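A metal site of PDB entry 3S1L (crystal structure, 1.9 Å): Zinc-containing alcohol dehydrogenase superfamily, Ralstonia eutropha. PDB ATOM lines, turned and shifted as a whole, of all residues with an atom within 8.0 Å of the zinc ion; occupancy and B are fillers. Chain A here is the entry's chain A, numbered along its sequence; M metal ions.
Merely in contact with the zinc ion: Gly 95. Along chain A the residues within 4 Å of the zinc ion span positions 94 to 108.
The zinc ion is bound by the side-chain sulfur (SG) of Cys 100, the side-chain sulfur (SG) of Cys 97, the side-chain sulfur (SG) of Cys 108 and the side-chain sulfur (SG) of Cys 94.
The side-chain sulfur (SG) of Cys 97 sits close to the backbone NH (N) of His 99, at 3.6 Å. The side-chain sulfur of Cys 108 lies close to the backbone NH of Lys 110 (3.4 Å). The side-chain sulfur (SG) of Cys 94 lies close to the backbone NH (N) of Tyr 96 (3.4 Å). The side-chain sulfur (SG) of Cys 100 lies close to the backbone NH (N) of Gly 95. The backbone carbonyl oxygen (O) of Cys 108 is in hydrogen-bond range of the side-chain amide nitrogen (NE2) of Gln 111, 3.0 Å away.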
ATOM      1  N   SER A  92     -16.123  19.079   7.671  1.00  0.00           N
ATOM      2  CA  SER A  92     -15.363  18.963   8.913  1.00  0.00           C
ATOM      3  C   SER A  92     -14.552  20.222   9.159  1.00  0.00           C
ATOM      4  O   SER A  92     -14.349  21.030   8.249  1.00  0.00           O
ATOM      5  CB  SER A  92     -14.417  17.765   8.844  1.00  0.00           C
ATOM      6  OG  SER A  92     -13.466  17.960   7.805  1.00  0.00           O
ATOM      7  N   ALA A  93     -14.076  20.377  10.388  1.00  0.00           N
ATOM      8  CA  ALA A  93     -13.179  21.460  10.754  1.00  0.00           C
ATOM      9  C   ALA A  93     -12.206  20.929  11.795  1.00  0.00           C
ATOM     10  O   ALA A  93     -12.440  19.845  12.345  1.00  0.00           O
ATOM     11  CB  ALA A  93     -13.965  22.647  11.295  1.00  0.00           C
ATOM     12  N   CYS A  94     -11.136  21.656  12.057  1.00  0.00           N
ATOM     13  CA  CYS A  94     -10.082  21.126  12.937  1.00  0.00           C
ATOM     14  C   CYS A  94     -10.561  20.930  14.364  1.00  0.00           C
ATOM     15  O   CYS A  94     -10.148  19.976  15.039  1.00  0.00           O
ATOM     16  CB  CYS A  94      -8.827  22.001  12.889  1.00  0.00           C
ATOM     17  SG  CYS A  94      -8.915  23.481  13.902  1.00  0.00           S
ATOM     18  N   GLY A  95     -11.412  21.832  14.834  1.00  0.00           N
ATOM     19  CA  GLY A  95     -12.004  21.714  16.164  1.00  0.00           C
ATOM     20  C   GLY A  95     -11.231  22.362  17.308  1.00  0.00           C
ATOM     21  O   GLY A  95     -11.679  22.301  18.458  1.00  0.00           O
ATOM     22  N   TYR A  96     -10.098  22.981  17.026  1.00  0.00           N
ATOM     23  CA  TYR A  96      -9.322  23.609  18.103  1.00  0.00           C
ATOM     24  C   TYR A  96      -8.625  24.918  17.720  1.00  0.00           C
ATOM     25  O   TYR A  96      -7.823  25.448  18.494  1.00  0.00           O
ATOM     26  CB  TYR A  96      -8.311  22.617  18.692  1.00  0.00           C
ATOM     27  CG  TYR A  96      -7.477  21.923  17.646  1.00  0.00           C
ATOM     28  CD1 TYR A  96      -6.574  22.630  16.869  1.00  0.00           C
ATOM     29  CD2 TYR A  96      -7.589  20.553  17.436  1.00  0.00           C
ATOM     30  CE1 TYR A  96      -5.806  22.006  15.911  1.00  0.00           C
ATOM     31  CE2 TYR A  96      -6.825  19.912  16.480  1.00  0.00           C
ATOM     32  CZ  TYR A  96      -5.931  20.647  15.717  1.00  0.00           C
ATOM     33  OH  TYR A  96      -5.167  20.006  14.761  1.00  0.00           O
ATOM     34  N   CYS A  97      -8.933  25.445  16.539  1.00  0.00           N
ATOM     35  CA  CYS A  97      -8.455  26.777  16.177  1.00  0.00           C
ATOM     36  C   CYS A  97      -9.336  27.789  16.885  1.00  0.00           C
ATOM     37  O   CYS A  97     -10.346  27.428  17.483  1.00  0.00           O
ATOM     38  CB  CYS A  97      -8.508  26.983  14.657  1.00  0.00           C
ATOM     39  SG  CYS A  97     -10.164  27.256  13.976  1.00  0.00           S
ATOM     40  N   GLU A  98      -8.958  29.068  16.826  1.00  0.00           N
ATOM     41  CA  GLU A  98      -9.729  30.091  17.520  1.00  0.00           C
ATOM     42  C   GLU A  98     -11.197  30.097  17.095  1.00  0.00           C
ATOM     43  O   GLU A  98     -12.089  30.147  17.931  1.00  0.00           O
ATOM     44  CB  GLU A  98      -9.100  31.463  17.324  1.00  0.00           C
ATOM     45  CG  GLU A  98      -9.769  32.564  18.107  1.00  0.00           C
ATOM     46  CD  GLU A  98      -8.978  33.853  18.103  1.00  0.00           C
ATOM     47  OE1 GLU A  98      -7.747  33.793  17.863  1.00  0.00           O
ATOM     48  OE2 GLU A  98      -9.570  34.921  18.350  1.00  0.00           O
ATOM     49  N   HIS A  99     -11.438  30.063  15.788  1.00  0.00           N
ATOM     50  CA  HIS A  99     -12.798  30.025  15.260  1.00  0.00           C
ATOM     51  C   HIS A  99     -13.581  28.834  15.800  1.00  0.00           C
ATOM     52  O   HIS A  99     -14.719  28.971  16.264  1.00  0.00           O
ATOM     53  CB  HIS A  99     -12.774  29.935  13.725  1.00  0.00           C
ATOM     54  CG  HIS A  99     -12.192  31.129  13.049  1.00  0.00           C
ATOM     55  ND1 HIS A  99     -12.601  32.422  13.315  1.00  0.00           N
ATOM     56  CD2 HIS A  99     -11.239  31.232  12.097  1.00  0.00           C
ATOM     57  CE1 HIS A  99     -11.923  33.267  12.563  1.00  0.00           C
ATOM     58  NE2 HIS A  99     -11.084  32.574  11.816  1.00  0.00           N
ATOM     59  N   CYS A 100     -12.985  27.653  15.720  1.00  0.00           N
ATOM     60  CA  CYS A 100     -13.643  26.431  16.155  1.00  0.00           C
ATOM     61  C   CYS A 100     -13.974  26.462  17.655  1.00  0.00           C
ATOM     62  O   CYS A 100     -15.043  26.021  18.065  1.00  0.00           O
ATOM     63  CB  CYS A 100     -12.787  25.205  15.819  1.00  0.00           C
ATOM     64  SG  CYS A 100     -12.817  24.739  14.050  1.00  0.00           S
ATOM     65  N   LEU A 101     -13.051  26.989  18.465  1.00  0.00           N
ATOM     66  CA  LEU A 101     -13.259  27.018  19.910  1.00  0.00           C
ATOM     67  C   LEU A 101     -14.320  28.023  20.330  1.00  0.00           C
ATOM     68  O   LEU A 101     -14.882  27.931  21.415  1.00  0.00           O
ATOM     69  CB  LEU A 101     -11.946  27.326  20.648  1.00  0.00           C
ATOM     70  CG  LEU A 101     -10.832  26.278  20.589  1.00  0.00           C
ATOM     71  CD1 LEU A 101      -9.673  26.689  21.491  1.00  0.00           C
ATOM     72  CD2 LEU A 101     -11.368  24.917  21.008  1.00  0.00           C
ATOM     73  N   TRP A 104     -17.468  29.169  15.881  1.00  0.00           N
ATOM     74  CA  TRP A 104     -17.549  29.707  14.527  1.00  0.00           C
ATOM     75  C   TRP A 104     -16.779  28.808  13.558  1.00  0.00           C
ATOM     76  O   TRP A 104     -15.987  29.291  12.736  1.00  0.00           O
ATOM     77  CB  TRP A 104     -16.996  31.137  14.491  1.00  0.00           C
ATOM     78  CG  TRP A 104     -18.001  32.198  14.880  1.00  0.00           C
ATOM     79  CD1 TRP A 104     -18.212  32.704  16.126  1.00  0.00           C
ATOM     80  CD2 TRP A 104     -18.926  32.862  14.008  1.00  0.00           C
ATOM     81  NE1 TRP A 104     -19.215  33.653  16.087  1.00  0.00           N
ATOM     82  CE2 TRP A 104     -19.664  33.771  14.804  1.00  0.00           C
ATOM     83  CE3 TRP A 104     -19.195  32.797  12.635  1.00  0.00           C
ATOM     84  CZ2 TRP A 104     -20.660  34.593  14.261  1.00  0.00           C
ATOM     85  CZ3 TRP A 104     -20.184  33.619  12.105  1.00  0.00           C
ATOM     86  CH2 TRP A 104     -20.899  34.495  12.920  1.00  0.00           C
ATOM     87  N   GLU A 105     -17.019  27.499  13.651  1.00  0.00           N
ATOM     88  CA  GLU A 105     -16.298  26.511  12.856  1.00  0.00           C
ATOM     89  C   GLU A 105     -16.487  26.724  11.358  1.00  0.00           C
ATOM     90  O   GLU A 105     -15.717  26.222  10.547  1.00  0.00           O
ATOM     91  CB  GLU A 105     -16.723  25.087  13.243  1.00  0.00           C
ATOM     92  CG  GLU A 105     -18.199  24.780  13.024  1.00  0.00           C
ATOM     93  CD  GLU A 105     -19.039  24.960  14.281  1.00  0.00           C
ATOM     94  OE1 GLU A 105     -18.675  25.785  15.141  1.00  0.00           O
ATOM     95  OE2 GLU A 105     -20.089  24.276  14.400  1.00  0.00           O
ATOM     96  N   THR A 106     -17.532  27.458  11.014  1.00  0.00           N
ATOM     97  CA  THR A 106     -17.822  27.782   9.632  1.00  0.00           C
ATOM     98  C   THR A 106     -16.697  28.627   9.014  1.00  0.00           C
ATOM     99  O   THR A 106     -16.586  28.731   7.790  1.00  0.00           O
ATOM    100  CB  THR A 106     -19.190  28.497   9.525  1.00  0.00           C
ATOM    101  OG1 THR A 106     -19.636  28.517   8.166  1.00  0.00           O
ATOM    102  CG2 THR A 106     -19.117  29.901  10.093  1.00  0.00           C
ATOM    103  N   LEU A 107     -15.868  29.225   9.863  1.00  0.00           N
ATOM    104  CA  LEU A 107     -14.767  30.070   9.414  1.00  0.00           C
ATOM    105  C   LEU A 107     -13.426  29.361   9.463  1.00  0.00           C
ATOM    106  O   LEU A 107     -12.392  29.953   9.132  1.00  0.00           O
ATOM    107  CB  LEU A 107     -14.700  31.346  10.254  1.00  0.00           C
ATOM    108  CG  LEU A 107     -15.945  32.246  10.240  1.00  0.00           C
ATOM    109  CD1 LEU A 107     -15.723  33.474  11.096  1.00  0.00           C
ATOM    110  CD2 LEU A 107     -16.295  32.625   8.813  1.00  0.00           C
ATOM    111  N   CYS A 108     -13.428  28.097   9.886  1.00  0.00           N
ATOM    112  CA  CYS A 108     -12.184  27.343  10.048  1.00  0.00           C
ATOM    113  C   CYS A 108     -11.351  27.304   8.764  1.00  0.00           C
ATOM    114  O   CYS A 108     -11.835  26.903   7.709  1.00  0.00           O
ATOM    115  CB  CYS A 108     -12.464  25.923  10.523  1.00  0.00           C
ATOM    116  SG  CYS A 108     -10.957  24.944  10.801  1.00  0.00           S
ATOM    117  N   GLU A 109     -10.093  27.704   8.881  1.00  0.00           N
ATOM    118  CA  GLU A 109      -9.202  27.708   7.720  1.00  0.00           C
ATOM    119  C   GLU A 109      -8.856  26.309   7.228  1.00  0.00           C
ATOM    120  O   GLU A 109      -8.500  26.132   6.063  1.00  0.00           O
ATOM    121  CB  GLU A 109      -7.923  28.500   8.041  1.00  0.00           C
ATOM    122  CG  GLU A 109      -8.137  29.996   8.098  1.00  0.00           C
ATOM    123  CD  GLU A 109      -6.873  30.757   8.436  1.00  0.00           C
ATOM    124  OE1 GLU A 109      -6.977  31.954   8.778  1.00  0.00           O
ATOM    125  OE2 GLU A 109      -5.781  30.161   8.345  1.00  0.00           O
ATOM    126  N   LYS A 110      -8.952  25.316   8.107  1.00  0.00           N
ATOM    127  CA  LYS A 110      -8.654  23.933   7.733  1.00  0.00           C
ATOM    128  C   LYS A 110      -9.894  23.118   7.380  1.00  0.00           C
ATOM    129  O   LYS A 110      -9.841  21.893   7.338  1.00  0.00           O
ATOM    130  CB  LYS A 110      -7.894  23.217   8.854  1.00  0.00           C
ATOM    131  CG  LYS A 110      -6.498  23.736   9.121  1.00  0.00           C
ATOM    132  CD  LYS A 110      -5.897  23.021  10.327  1.00  0.00           C
ATOM    133  CE  LYS A 110      -4.540  23.602  10.715  1.00  0.00           C
ATOM    134  NZ  LYS A 110      -4.042  23.017  11.990  1.00  0.00           N
ATOM    135  N   GLN A 111     -11.017  23.790   7.130  1.00  0.00           N
ATOM    136  CA  GLN A 111     -12.260  23.068   6.862  1.00  0.00           C
ATOM    137  C   GLN A 111     -12.212  22.293   5.553  1.00  0.00           C
ATOM    138  O   GLN A 111     -11.537  22.695   4.593  1.00  0.00           O
ATOM    139  CB  GLN A 111     -13.468  24.007   6.885  1.00  0.00           C
ATOM    140  CG  GLN A 111     -13.615  24.893   5.655  1.00  0.00           C
ATOM    141  CD  GLN A 111     -14.764  25.879   5.791  1.00  0.00           C
ATOM    142  OE1 GLN A 111     -15.862  25.642   5.289  1.00  0.00           O
ATOM    143  NE2 GLN A 111     -14.513  26.993   6.474  1.00  0.00           N
ATOM    144  N   TYR A 132     -20.048  16.498  12.355  1.00  0.00           N
ATOM    145  CA  TYR A 132     -20.462  17.652  11.560  1.00  0.00           C
ATOM    146  C   TYR A 132     -21.719  17.433  10.717  1.00  0.00           C
ATOM    147  O   TYR A 132     -22.180  18.362  10.045  1.00  0.00           O
ATOM    148  CB  TYR A 132     -19.307  18.142  10.683  1.00  0.00           C
ATOM    149  CG  TYR A 132     -18.183  18.695  11.509  1.00  0.00           C
ATOM    150  CD1 TYR A 132     -17.190  17.856  11.995  1.00  0.00           C
ATOM    151  CD2 TYR A 132     -18.143  20.036  11.866  1.00  0.00           C
ATOM    152  CE1 TYR A 132     -16.173  18.344  12.784  1.00  0.00           C
ATOM    153  CE2 TYR A 132     -17.123  20.535  12.662  1.00  0.00           C
ATOM    154  CZ  TYR A 132     -16.140  19.682  13.105  1.00  0.00           C
ATOM    155  OH  TYR A 132     -15.126  20.153  13.896  1.00  0.00           O
HETATM  156 ZN    ZN M   1     -10.679  25.096  13.150  1.00  0.00          ZN
